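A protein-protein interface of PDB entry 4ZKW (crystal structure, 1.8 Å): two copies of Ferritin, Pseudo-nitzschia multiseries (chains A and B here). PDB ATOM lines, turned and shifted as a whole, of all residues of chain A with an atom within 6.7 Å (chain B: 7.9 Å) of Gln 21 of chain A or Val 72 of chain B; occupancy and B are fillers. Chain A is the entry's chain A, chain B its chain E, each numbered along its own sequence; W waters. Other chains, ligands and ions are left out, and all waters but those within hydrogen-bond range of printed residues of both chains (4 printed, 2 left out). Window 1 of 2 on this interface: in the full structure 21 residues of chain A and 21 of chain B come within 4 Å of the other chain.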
ATOM      1  N   GLU A  16      27.346  -2.572  30.089  1.00  0.00           N
ATOM      2  CA  GLU A  16      26.421  -1.713  29.330  1.00  0.00           C
ATOM      3  C   GLU A  16      25.839  -2.505  28.206  1.00  0.00           C
ATOM      4  O   GLU A  16      24.621  -2.492  27.978  1.00  0.00           O
ATOM      5  CB  GLU A  16      27.118  -0.450  28.785  1.00  0.00           C
ATOM      6  CG  GLU A  16      27.680   0.419  29.849  1.00  0.00           C
ATOM      7  CD  GLU A  16      26.624   1.053  30.757  1.00  0.00           C
ATOM      8  OE1 GLU A  16      25.460   1.160  30.350  1.00  0.00           O
ATOM      9  OE2 GLU A  16      26.965   1.305  31.923  1.00  0.00           O
ATOM     10  N   PHE A  17      26.670  -3.224  27.461  1.00  0.00           N
ATOM     11  CA  PHE A  17      26.149  -4.059  26.342  1.00  0.00           C
ATOM     12  C   PHE A  17      25.298  -5.252  26.778  1.00  0.00           C
ATOM     13  O   PHE A  17      24.314  -5.627  26.068  1.00  0.00           O
ATOM     14  CB  PHE A  17      27.292  -4.501  25.435  1.00  0.00           C
ATOM     15  CG  PHE A  17      27.987  -3.379  24.738  1.00  0.00           C
ATOM     16  CD1 PHE A  17      27.349  -2.173  24.427  1.00  0.00           C
ATOM     17  CD2 PHE A  17      29.338  -3.531  24.331  1.00  0.00           C
ATOM     18  CE1 PHE A  17      28.000  -1.182  23.718  1.00  0.00           C
ATOM     19  CE2 PHE A  17      29.982  -2.501  23.651  1.00  0.00           C
ATOM     20  CZ  PHE A  17      29.326  -1.313  23.377  1.00  0.00           C
ATOM     21  N   THR A  18      25.643  -5.848  27.931  1.00  0.00           N
ATOM     22  CA  THR A  18      24.868  -6.899  28.490  1.00  0.00           C
ATOM     23  C   THR A  18      23.471  -6.275  28.778  1.00  0.00           C
ATOM     24  O   THR A  18      22.434  -6.904  28.491  1.00  0.00           O
ATOM     25  CB  THR A  18      25.524  -7.446  29.810  1.00  0.00           C
ATOM     26  OG1 THR A  18      26.793  -8.022  29.498  1.00  0.00           O
ATOM     27  CG2 THR A  18      24.625  -8.467  30.519  1.00  0.00           C
ATOM     28  N   ALA A  19      23.460  -5.119  29.406  1.00  0.00           N
ATOM     29  CA  ALA A  19      22.150  -4.516  29.786  1.00  0.00           C
ATOM     30  C   ALA A  19      21.340  -4.218  28.511  1.00  0.00           C
ATOM     31  O   ALA A  19      20.116  -4.469  28.488  1.00  0.00           O
ATOM     32  CB  ALA A  19      22.352  -3.260  30.664  1.00  0.00           C
ATOM     33  N   SER A  20      21.991  -3.659  27.465  1.00  0.00           N
ATOM     34  CA  SER A  20      21.326  -3.458  26.185  1.00  0.00           C
ATOM     35  C   SER A  20      20.641  -4.728  25.706  1.00  0.00           C
ATOM     36  O   SER A  20      19.508  -4.701  25.261  1.00  0.00           O
ATOM     37  CB  SER A  20      22.293  -2.940  25.176  1.00  0.00           C
ATOM     38  OG  SER A  20      21.735  -2.721  23.930  1.00  0.00           O
ATOM     39  N   GLN A  21      21.321  -5.891  25.764  1.00  0.00           N
ATOM     40  CA  GLN A  21      20.754  -7.098  25.282  1.00  0.00           C
ATOM     41  C   GLN A  21      19.627  -7.591  26.208  1.00  0.00           C
ATOM     42  O   GLN A  21      18.691  -8.188  25.693  1.00  0.00           O
ATOM     43  CB  GLN A  21      21.872  -8.201  25.162  1.00  0.00           C
ATOM     44  CG  GLN A  21      22.726  -8.001  23.946  1.00  0.00           C
ATOM     45  CD  GLN A  21      21.943  -8.337  22.659  1.00  0.00           C
ATOM     46  OE1 GLN A  21      21.373  -7.453  22.022  1.00  0.00           O
ATOM     47  NE2 GLN A  21      21.905  -9.598  22.310  1.00  0.00           N
ATOM     48  N   VAL A  22      19.714  -7.338  27.513  1.00  0.00           N
ATOM     49  CA  VAL A  22      18.663  -7.786  28.422  1.00  0.00           C
ATOM     50  C   VAL A  22      17.374  -6.935  28.171  1.00  0.00           C
ATOM     51  O   VAL A  22      16.328  -7.480  28.056  1.00  0.00           O
ATOM     52  CB  VAL A  22      19.053  -7.670  29.866  1.00  0.00           C
ATOM     53  CG1 VAL A  22      17.870  -7.920  30.765  1.00  0.00           C
ATOM     54  CG2 VAL A  22      20.161  -8.674  30.175  1.00  0.00           C
ATOM     55  N   TYR A  23      17.545  -5.661  27.955  1.00  0.00           N
ATOM     56  CA  TYR A  23      16.422  -4.810  27.512  1.00  0.00           C
ATOM     57  C   TYR A  23      15.834  -5.290  26.219  1.00  0.00           C
ATOM     58  O   TYR A  23      14.593  -5.325  26.081  1.00  0.00           O
ATOM     59  CB  TYR A  23      16.894  -3.325  27.456  1.00  0.00           C
ATOM     60  CG  TYR A  23      16.791  -2.568  28.730  1.00  0.00           C
ATOM     61  CD1 TYR A  23      15.550  -2.175  29.217  1.00  0.00           C
ATOM     62  CD2 TYR A  23      17.926  -2.188  29.466  1.00  0.00           C
ATOM     63  CE1 TYR A  23      15.436  -1.470  30.386  1.00  0.00           C
ATOM     64  CE2 TYR A  23      17.813  -1.478  30.642  1.00  0.00           C
ATOM     65  CZ  TYR A  23      16.566  -1.085  31.081  1.00  0.00           C
ATOM     66  OH  TYR A  23      16.415  -0.356  32.237  1.00  0.00           O
ATOM     67  N   LEU A  24      16.639  -5.688  25.209  1.00  0.00           N
ATOM     68  CA  LEU A  24      16.103  -6.226  24.014  1.00  0.00           C
ATOM     69  C   LEU A  24      15.304  -7.492  24.290  1.00  0.00           C
ATOM     70  O   LEU A  24      14.179  -7.678  23.705  1.00  0.00           O
ATOM     71  CB  LEU A  24      17.139  -6.434  22.936  1.00  0.00           C
ATOM     72  CG  LEU A  24      16.691  -7.035  21.609  1.00  0.00           C
ATOM     73  CD1 LEU A  24      15.776  -6.014  20.894  1.00  0.00           C
ATOM     74  CD2 LEU A  24      17.907  -7.335  20.729  1.00  0.00           C
ATOM     75  N   SER A  25      15.814  -8.391  25.141  1.00  0.00           N
ATOM     76  CA  SER A  25      15.035  -9.588  25.522  1.00  0.00           C
ATOM     77  C   SER A  25      13.711  -9.231  26.214  1.00  0.00           C
ATOM     78  O   SER A  25      12.699  -9.890  26.031  1.00  0.00           O
ATOM     79  CB  SER A  25      15.853 -10.542  26.394  1.00  0.00           C
ATOM     80  OG  SER A  25      16.048 -10.011  27.707  1.00  0.00           O
ATOM     81  N   ALA A  26      13.710  -8.168  26.975  1.00  0.00           N
ATOM     82  CA  ALA A  26      12.438  -7.694  27.599  1.00  0.00           C
ATOM     83  C   ALA A  26      11.471  -7.227  26.490  1.00  0.00           C
ATOM     84  O   ALA A  26      10.289  -7.569  26.542  1.00  0.00           O
ATOM     85  CB  ALA A  26      12.669  -6.661  28.593  1.00  0.00           C
ATOM     86  N   ILE A  28      11.267  -8.261  23.413  1.00  0.00           N
ATOM     87  CA  ILE A  28      10.792  -9.381  22.736  1.00  0.00           C
ATOM     88  C   ILE A  28       9.682 -10.075  23.498  1.00  0.00           C
ATOM     89  O   ILE A  28       8.682 -10.457  22.918  1.00  0.00           O
ATOM     90  CB  ILE A  28      11.975 -10.351  22.444  1.00  0.00           C
ATOM     91  CG1 ILE A  28      12.923  -9.728  21.429  1.00  0.00           C
ATOM     92  CG2 ILE A  28      11.467 -11.663  21.954  1.00  0.00           C
ATOM     93  CD1 ILE A  28      14.301 -10.432  21.266  1.00  0.00           C
ATOM     94  N   SER A  46      17.070  -0.226  25.493  1.00  0.00           N
ATOM     95  CA  SER A  46      18.146  -0.992  24.887  1.00  0.00           C
ATOM     96  C   SER A  46      19.150  -0.185  24.066  1.00  0.00           C
ATOM     97  O   SER A  46      20.406  -0.351  24.171  1.00  0.00           O
ATOM     98  CB  SER A  46      17.569  -2.113  24.042  1.00  0.00           C
ATOM     99  OG  SER A  46      18.572  -2.915  23.346  1.00  0.00           O
ATOM    100  N   GLU A  49      21.268   2.118  26.435  1.00  0.00           N
ATOM    101  CA  GLU A  49      22.350   1.406  27.113  1.00  0.00           C
ATOM    102  C   GLU A  49      23.491   1.110  26.192  1.00  0.00           C
ATOM    103  O   GLU A  49      24.641   1.191  26.612  1.00  0.00           O
ATOM    104  CB  GLU A  49      21.846   0.079  27.670  1.00  0.00           C
ATOM    105  CG  GLU A  49      20.781   0.224  28.690  1.00  0.00           C
ATOM    106  CD  GLU A  49      21.290   0.485  30.067  1.00  0.00           C
ATOM    107  OE1 GLU A  49      22.505   0.764  30.255  1.00  0.00           O
ATOM    108  OE2 GLU A  49      20.448   0.441  30.945  1.00  0.00           O
ATOM    109  N   GLN A  70      34.441  -8.062  25.018  1.00  0.00           N
ATOM    110  CA  GLN A  70      34.089  -9.402  25.485  1.00  0.00           C
ATOM    111  C   GLN A  70      32.782  -9.853  24.915  1.00  0.00           C
ATOM    112  O   GLN A  70      32.044  -9.033  24.353  1.00  0.00           O
ATOM    113  CB  GLN A  70      34.034  -9.382  26.960  1.00  0.00           C
ATOM    114  CG  GLN A  70      35.298  -8.773  27.519  1.00  0.00           C
ATOM    115  CD  GLN A  70      35.277  -8.610  29.010  1.00  0.00           C
ATOM    116  OE1 GLN A  70      34.297  -8.152  29.630  1.00  0.00           O
ATOM    117  NE2 GLN A  70      36.412  -8.917  29.611  1.00  0.00           N
ATOM    118  N   ALA A  71      32.501 -11.160  25.007  1.00  0.00           N
ATOM    119  CA  ALA A  71      31.246 -11.664  24.587  1.00  0.00           C
ATOM    120  C   ALA A  71      30.131 -10.940  25.390  1.00  0.00           C
ATOM    121  O   ALA A  71      30.293 -10.588  26.593  1.00  0.00           O
ATOM    122  CB  ALA A  71      31.132 -13.157  24.842  1.00  0.00           C
ATOM    123  N   VAL A  72      29.037 -10.765  24.713  1.00  0.00           N
ATOM    124  CA  VAL A  72      27.780 -10.338  25.369  1.00  0.00           C
ATOM    125  C   VAL A  72      26.906 -11.532  25.595  1.00  0.00           C
ATOM    126  O   VAL A  72      26.472 -12.154  24.666  1.00  0.00           O
ATOM    127  CB  VAL A  72      27.038  -9.255  24.558  1.00  0.00           C
ATOM    128  CG1 VAL A  72      25.878  -8.724  25.404  1.00  0.00           C
ATOM    129  CG2 VAL A  72      28.010  -8.133  24.196  1.00  0.00           C
ATOM    130  N   PRO A  73      26.716 -11.903  26.866  1.00  0.00           N
ATOM    131  CA  PRO A  73      26.149 -13.227  27.121  1.00  0.00           C
ATOM    132  C   PRO A  73      24.689 -13.182  26.771  1.00  0.00           C
ATOM    133  O   PRO A  73      24.079 -12.060  26.797  1.00  0.00           O
ATOM    134  CB  PRO A  73      26.300 -13.425  28.647  1.00  0.00           C
ATOM    135  CG  PRO A  73      26.450 -12.058  29.186  1.00  0.00           C
ATOM    136  CD  PRO A  73      27.179 -11.275  28.115  1.00  0.00           C
ATOM    137  N   ALA A  74      24.183 -14.328  26.434  1.00  0.00           N
ATOM    138  CA  ALA A  74      22.725 -14.523  26.180  1.00  0.00           C
ATOM    139  C   ALA A  74      21.910 -14.135  27.381  1.00  0.00           C
ATOM    140  O   ALA A  74      22.286 -14.398  28.544  1.00  0.00           O
ATOM    141  CB  ALA A  74      22.444 -15.887  25.809  1.00  0.00           C
ATOM    142  N   PRO A  75      20.834 -13.394  27.154  1.00  0.00           N
ATOM    143  CA  PRO A  75      19.996 -12.985  28.292  1.00  0.00           C
ATOM    144  C   PRO A  75      19.317 -14.211  28.877  1.00  0.00           C
ATOM    145  O   PRO A  75      18.920 -15.042  28.124  1.00  0.00           O
ATOM    146  CB  PRO A  75      18.928 -12.070  27.623  1.00  0.00           C
ATOM    147  CG  PRO A  75      19.692 -11.424  26.486  1.00  0.00           C
ATOM    148  CD  PRO A  75      20.599 -12.552  25.938  1.00  0.00           C
ATOM    149  N   VAL B  13      19.681 -13.353  13.189  1.00  0.00           N
ATOM    150  CA  VAL B  13      19.746 -12.375  14.257  1.00  0.00           C
ATOM    151  C   VAL B  13      21.121 -12.331  14.918  1.00  0.00           C
ATOM    152  O   VAL B  13      21.793 -11.283  15.009  1.00  0.00           O
ATOM    153  CB  VAL B  13      18.620 -12.528  15.293  1.00  0.00           C
ATOM    154  CG1 VAL B  13      18.814 -11.570  16.429  1.00  0.00           C
ATOM    155  CG2 VAL B  13      17.264 -12.379  14.597  1.00  0.00           C
ATOM    156  N   THR B  14      21.577 -13.511  15.368  1.00  0.00           N
ATOM    157  CA  THR B  14      22.932 -13.623  15.899  1.00  0.00           C
ATOM    158  C   THR B  14      24.015 -13.114  14.916  1.00  0.00           C
ATOM    159  O   THR B  14      24.943 -12.396  15.354  1.00  0.00           O
ATOM    160  CB  THR B  14      23.225 -15.095  16.270  1.00  0.00           C
ATOM    161  OG1 THR B  14      22.180 -15.525  17.156  1.00  0.00           O
ATOM    162  CG2 THR B  14      24.589 -15.198  16.931  1.00  0.00           C
ATOM    163  N   GLN B  15      23.925 -13.422  13.638  1.00  0.00           N
ATOM    164  CA  GLN B  15      24.954 -12.995  12.716  1.00  0.00           C
ATOM    165  C   GLN B  15      24.951 -11.445  12.568  1.00  0.00           C
ATOM    166  O   GLN B  15      26.028 -10.843  12.477  1.00  0.00           O
ATOM    167  CB  GLN B  15      24.810 -13.661  11.348  1.00  0.00           C
ATOM    168  CG  GLN B  15      25.810 -13.153  10.276  1.00  0.00           C
ATOM    169  CD  GLN B  15      27.293 -13.501  10.566  1.00  0.00           C
ATOM    170  OE1 GLN B  15      28.269 -12.735  10.227  1.00  0.00           O
ATOM    171  NE2 GLN B  15      27.465 -14.616  11.270  1.00  0.00           N
ATOM    172  N   GLU B  16      23.781 -10.824  12.601  1.00  0.00           N
ATOM    173  CA  GLU B  16      23.733  -9.356  12.493  1.00  0.00           C
ATOM    174  C   GLU B  16      24.358  -8.741  13.695  1.00  0.00           C
ATOM    175  O   GLU B  16      25.125  -7.835  13.570  1.00  0.00           O
ATOM    176  CB  GLU B  16      22.293  -8.781  12.343  1.00  0.00           C
ATOM    177  CG  GLU B  16      21.536  -9.335  11.190  1.00  0.00           C
ATOM    178  CD  GLU B  16      22.069  -8.854   9.829  1.00  0.00           C
ATOM    179  OE1 GLU B  16      22.828  -7.873   9.727  1.00  0.00           O
ATOM    180  OE2 GLU B  16      21.814  -9.554   8.834  1.00  0.00           O
ATOM    181  N   PHE B  17      24.064  -9.225  14.902  1.00  0.00           N
ATOM    182  CA  PHE B  17      24.618  -8.632  16.095  1.00  0.00           C
ATOM    183  C   PHE B  17      26.140  -8.919  16.256  1.00  0.00           C
ATOM    184  O   PHE B  17      26.880  -8.130  16.791  1.00  0.00           O
ATOM    185  CB  PHE B  17      23.857  -9.093  17.304  1.00  0.00           C
ATOM    186  CG  PHE B  17      22.419  -8.574  17.376  1.00  0.00           C
ATOM    187  CD1 PHE B  17      22.017  -7.430  16.725  1.00  0.00           C
ATOM    188  CD2 PHE B  17      21.491  -9.235  18.118  1.00  0.00           C
ATOM    189  CE1 PHE B  17      20.733  -6.945  16.855  1.00  0.00           C
ATOM    190  CE2 PHE B  17      20.169  -8.809  18.164  1.00  0.00           C
ATOM    191  CZ  PHE B  17      19.793  -7.642  17.543  1.00  0.00           C
ATOM    192  N   THR B  18      26.563 -10.115  15.814  1.00  0.00           N
ATOM    193  CA  THR B  18      27.983 -10.431  15.732  1.00  0.00           C
ATOM    194  C   THR B  18      28.698  -9.480  14.812  1.00  0.00           C
ATOM    195  O   THR B  18      29.777  -8.978  15.168  1.00  0.00           O
ATOM    196  CB  THR B  18      28.174 -11.859  15.207  1.00  0.00           C
ATOM    197  OG1 THR B  18      27.549 -12.765  16.114  1.00  0.00           O
ATOM    198  CG2 THR B  18      29.666 -12.202  15.061  1.00  0.00           C
ATOM    199  N   ALA B  19      28.164  -9.286  13.635  1.00  0.00           N
ATOM    200  CA  ALA B  19      28.708  -8.296  12.710  1.00  0.00           C
ATOM    201  C   ALA B  19      28.763  -6.896  13.283  1.00  0.00           C
ATOM    202  O   ALA B  19      29.754  -6.210  13.128  1.00  0.00           O
ATOM    203  CB  ALA B  19      27.949  -8.281  11.375  1.00  0.00           C
ATOM    204  N   SER B  20      27.700  -6.465  13.963  1.00  0.00           N
ATOM    205  CA  SER B  20      27.730  -5.218  14.660  1.00  0.00           C
ATOM    206  C   SER B  20      28.928  -5.062  15.632  1.00  0.00           C
ATOM    207  O   SER B  20      29.608  -4.014  15.644  1.00  0.00           O
ATOM    208  CB  SER B  20      26.377  -4.958  15.370  1.00  0.00           C
ATOM    209  OG  SER B  20      26.449  -3.755  16.095  1.00  0.00           O
ATOM    210  N   GLN B  21      29.226  -6.110  16.386  1.00  0.00           N
ATOM    211  CA  GLN B  21      30.345  -6.110  17.334  1.00  0.00           C
ATOM    212  C   GLN B  21      31.704  -6.158  16.621  1.00  0.00           C
ATOM    213  O   GLN B  21      32.642  -5.458  17.054  1.00  0.00           O
ATOM    214  CB  GLN B  21      30.260  -7.272  18.315  1.00  0.00           C
ATOM    215  CG  GLN B  21      29.225  -7.199  19.372  1.00  0.00           C
ATOM    216  CD  GLN B  21      29.521  -6.033  20.314  1.00  0.00           C
ATOM    217  OE1 GLN B  21      29.055  -4.921  20.068  1.00  0.00           O
ATOM    218  NE2 GLN B  21      30.246  -6.296  21.373  1.00  0.00           N
ATOM    219  N   VAL B  22      31.764  -6.860  15.506  1.00  0.00           N
ATOM    220  CA  VAL B  22      33.028  -6.860  14.718  1.00  0.00           C
ATOM    221  C   VAL B  22      33.349  -5.485  14.157  1.00  0.00           C
ATOM    222  O   VAL B  22      34.468  -4.977  14.238  1.00  0.00           O
ATOM    223  CB  VAL B  22      33.031  -7.863  13.619  1.00  0.00           C
ATOM    224  CG1 VAL B  22      34.252  -7.672  12.731  1.00  0.00           C
ATOM    225  CG2 VAL B  22      32.982  -9.272  14.206  1.00  0.00           C
ATOM    226  N   ARG B  50      23.332  -3.550  13.687  1.00  0.00           N
ATOM    227  CA  ARG B  50      22.415  -3.751  14.794  1.00  0.00           C
ATOM    228  C   ARG B  50      20.967  -3.437  14.339  1.00  0.00           C
ATOM    229  O   ARG B  50      20.019  -4.211  14.647  1.00  0.00           O
ATOM    230  CB  ARG B  50      22.798  -2.934  15.990  1.00  0.00           C
ATOM    231  CG  ARG B  50      21.784  -3.069  17.154  1.00  0.00           C
ATOM    232  CD  ARG B  50      22.355  -2.437  18.391  1.00  0.00           C
ATOM    233  NE  ARG B  50      21.449  -2.588  19.529  1.00  0.00           N
ATOM    234  CZ  ARG B  50      20.410  -1.770  19.662  1.00  0.00           C
ATOM    235  NH1 ARG B  50      20.238  -0.814  18.785  1.00  0.00           N
ATOM    236  NH2 ARG B  50      19.553  -1.933  20.631  1.00  0.00           N
ATOM    237  N   LEU B  54      17.647  -5.856  14.492  1.00  0.00           N
ATOM    238  CA  LEU B  54      16.377  -5.425  15.101  1.00  0.00           C
ATOM    239  C   LEU B  54      15.216  -5.624  14.087  1.00  0.00           C
ATOM    240  O   LEU B  54      14.110  -5.977  14.488  1.00  0.00           O
ATOM    241  CB  LEU B  54      16.400  -3.969  15.596  1.00  0.00           C
ATOM    242  CG  LEU B  54      17.399  -3.750  16.724  1.00  0.00           C
ATOM    243  CD1 LEU B  54      17.314  -2.273  17.079  1.00  0.00           C
ATOM    244  CD2 LEU B  54      17.094  -4.620  17.904  1.00  0.00           C
ATOM    245  N   LEU B  69      17.622 -14.891  21.952  1.00  0.00           N
ATOM    246  CA  LEU B  69      18.862 -14.152  21.808  1.00  0.00           C
ATOM    247  C   LEU B  69      20.021 -15.035  22.329  1.00  0.00           C
ATOM    248  O   LEU B  69      19.966 -15.492  23.459  1.00  0.00           O
ATOM    249  CB  LEU B  69      18.798 -12.840  22.550  1.00  0.00           C
ATOM    250  CG  LEU B  69      17.827 -11.789  21.923  1.00  0.00           C
ATOM    251  CD1 LEU B  69      17.878 -10.560  22.757  1.00  0.00           C
ATOM    252  CD2 LEU B  69      18.164 -11.548  20.458  1.00  0.00           C
ATOM    253  N   GLN B  70      21.029 -15.179  21.493  1.00  0.00           N
ATOM    254  CA  GLN B  70      22.200 -15.996  21.742  1.00  0.00           C
ATOM    255  C   GLN B  70      23.311 -15.059  22.172  1.00  0.00           C
ATOM    256  O   GLN B  70      23.206 -13.815  22.126  1.00  0.00           O
ATOM    257  CB  GLN B  70      22.563 -16.793  20.504  1.00  0.00           C
ATOM    258  CG  GLN B  70      21.435 -17.737  20.105  1.00  0.00           C
ATOM    259  CD  GLN B  70      21.423 -19.017  20.924  1.00  0.00           C
ATOM    260  OE1 GLN B  70      22.399 -19.774  20.922  1.00  0.00           O
ATOM    261  NE2 GLN B  70      20.322 -19.269  21.615  1.00  0.00           N
ATOM    262  N   ALA B  71      24.358 -15.641  22.751  1.00  0.00           N
ATOM    263  CA  ALA B  71      25.514 -14.874  23.033  1.00  0.00           C
ATOM    264  C   ALA B  71      26.027 -14.217  21.772  1.00  0.00           C
ATOM    265  O   ALA B  71      25.984 -14.827  20.722  1.00  0.00           O
ATOM    266  CB  ALA B  71      26.598 -15.802  23.593  1.00  0.00           C
ATOM    267  N   VAL B  72      26.560 -13.012  21.945  1.00  0.00           N
ATOM    268  CA  VAL B  72      27.278 -12.328  20.883  1.00  0.00           C
ATOM    269  C   VAL B  72      28.768 -12.539  21.166  1.00  0.00           C
ATOM    270  O   VAL B  72      29.279 -12.076  22.134  1.00  0.00           O
ATOM    271  CB  VAL B  72      26.945 -10.863  20.789  1.00  0.00           C
ATOM    272  CG1 VAL B  72      27.544 -10.288  19.492  1.00  0.00           C
ATOM    273  CG2 VAL B  72      25.404 -10.631  20.760  1.00  0.00           C
ATOM    274  N   PRO B  73      29.426 -13.313  20.288  1.00  0.00           N
ATOM    275  CA  PRO B  73      30.786 -13.691  20.639  1.00  0.00           C
ATOM    276  C   PRO B  73      31.780 -12.514  20.643  1.00  0.00           C
ATOM    277  O   PRO B  73      31.592 -11.494  19.926  1.00  0.00           O
ATOM    278  CB  PRO B  73      31.149 -14.762  19.600  1.00  0.00           C
ATOM    279  CG  PRO B  73      30.161 -14.619  18.495  1.00  0.00           C
ATOM    280  CD  PRO B  73      28.975 -13.862  19.022  1.00  0.00           C
ATOM    281  N   ALA B  74      32.804 -12.646  21.463  1.00  0.00           N
ATOM    282  CA  ALA B  74      33.909 -11.670  21.435  1.00  0.00           C
ATOM    283  C   ALA B  74      34.600 -11.609  20.047  1.00  0.00           C
ATOM    284  O   ALA B  74      34.921 -12.632  19.430  1.00  0.00           O
ATOM    285  CB  ALA B  74      34.911 -11.952  22.550  1.00  0.00           C
ATOM    286  N   PRO B  75      34.823 -10.399  19.514  1.00  0.00           N
ATOM    287  CA  PRO B  75      35.486 -10.272  18.216  1.00  0.00           C
ATOM    288  C   PRO B  75      36.930 -10.759  18.442  1.00  0.00           C
ATOM    289  O   PRO B  75      37.449 -10.504  19.485  1.00  0.00           O
ATOM    290  CB  PRO B  75      35.474  -8.764  17.955  1.00  0.00           C
ATOM    291  CG  PRO B  75      34.179  -8.325  18.652  1.00  0.00           C
ATOM    292  CD  PRO B  75      34.210  -9.093  19.952  1.00  0.00           C
HETATM  293  O   HOH W   1      31.239  -6.297  24.423  1.00  0.00           O
HETATM  294  O   HOH W   2      21.157  -4.481  21.882  1.00  0.00           O
HETATM  295  O   HOH W   3      22.011 -11.912  20.185  1.00  0.00           O
HETATM  296  O   HOH W   4      17.945 -15.002  25.738  1.00  0.00           O
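Gln 21 of chain A touches Val 72 of chain B, but with the chains exchanged Val 72 of chain A does not touch Gln 21 of chain B (4.04 Å).
Gln 70 of chain A touches Ala 74 of chain B, and with the chains exchanged Ala 74 of chain A touches Gln 70 of chain B.
Ala 71 of chain A touches Val 72 of chain B, and with the chains exchanged Val 72 of chain A touches Ala 71 of chain B.
Val 72 of chain B touches its own counterpart, Val 72 of chain A.
Positions printed for both chains: 16, 17, 18, 19, 20, 21, 22, 70, 71, 72, 73, 74 and 75.
Of the 17 pairs that touch across the chains among the printed residues, 7 have their exchanged pair printed and touching as well.
The side-chain hydroxyl (OG) of Ser 20 of chain A lies within hydrogen-bond range of the backbone carbonyl oxygen (O) of Ser 46 of chain A (2.7 Å).
O of Val 22 of chain A sits at hydrogen-bond distance from OG of Ser 25 of chain A (2.6 Å).
Water W4 bridges the backbone carbonyl oxygen of Pro 75 of chain A and the backbone carbonyl oxygen of Leu 69 of chain B.
Water W2 lies within hydrogen-bond range of OG of Ser 20 of chain A, OE1 of Gln 21 of chain A, NE of Arg 50 of chain B and OG of Ser 46 of chain A.
Water W1 bridges O of Gln 70 of chain A (2.9 Å) and NE2 of Gln 21 of chain B (3.2 Å).
Water W3 bridges the backbone carbonyl oxygen (O) of Gln 70 of chain B (3.0 Å) and the side-chain amide nitrogen (NE2) of Gln 21 of chain A (3.1 Å).
The side-chain hydroxyl (OG) of Ser 46 of chain A lies within hydrogen-bond range of the guanidinium group (NH2) of Arg 50 of chain B.
O of Val 72 of chain A is in hydrogen-bond range of N of Val 72 of chain B, 2.9 Å away.
O of Gln 21 of chain A touches CD1 of Leu 69 of chain B (3.9 Å).
CZ of Phe 17 of chain B touches CD2 of Leu 24 of chain A, 3.7 Å away.
Leu 24 of chain A touches Leu 54 of chain B.
CD1 of Leu 69 of chain B touches CD2 of Leu 24 of chain A (3.8 Å).
Ile 28 of chain A touches Leu 69 of chain B.
Ala 74 of chain B touches Gln 70 of chain A (CB to C, 3.8 Å).
Ala 71 of chain A touches Val 72 of chain B.
N of Ala 71 of chain A touches CB of Ala 74 of chain B, 3.5 Å away.
Ala 71 of chain B touches Val 72 of chain A.
CB of Ala 74 of chain A touches C of Gln 70 of chain B (3.8 Å).
Hydrophobic or aromatic side chains of chain A that line the printed part of chain B: Leu 24, Ile 28, Ala 71, Ala 74 and Pro 75.
Hydrophobic or aromatic side chains of chain B that line the printed part of chain A: Phe 17, Leu 54, Leu 69, Ala 71, Val 72 and Ala 74.
Among the printed residues, no Asp or Glu carboxylate lies within 4 Å of a Lys or Arg side-chain nitrogen of the other chain.
Printed residues of chain A within 4 Å of Val 72 of chain B: Gln 21 (3.96 Å), Ala 71 (3.2 Å) and Val 72 (2.9 Å).
Printed residues of chain B within 4 Å of Ala 71 of chain A: Val 72 and Ala 74.
Printed residues of chain B within 4 Å of Ser 46 of chain A: Arg 50.
Val 13 of chain B touches none of the printed residues of chain A.
The nearest residue of chain A that does not touch Val 72 of chain B is Gln 70 of chain A (4.7 Å).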
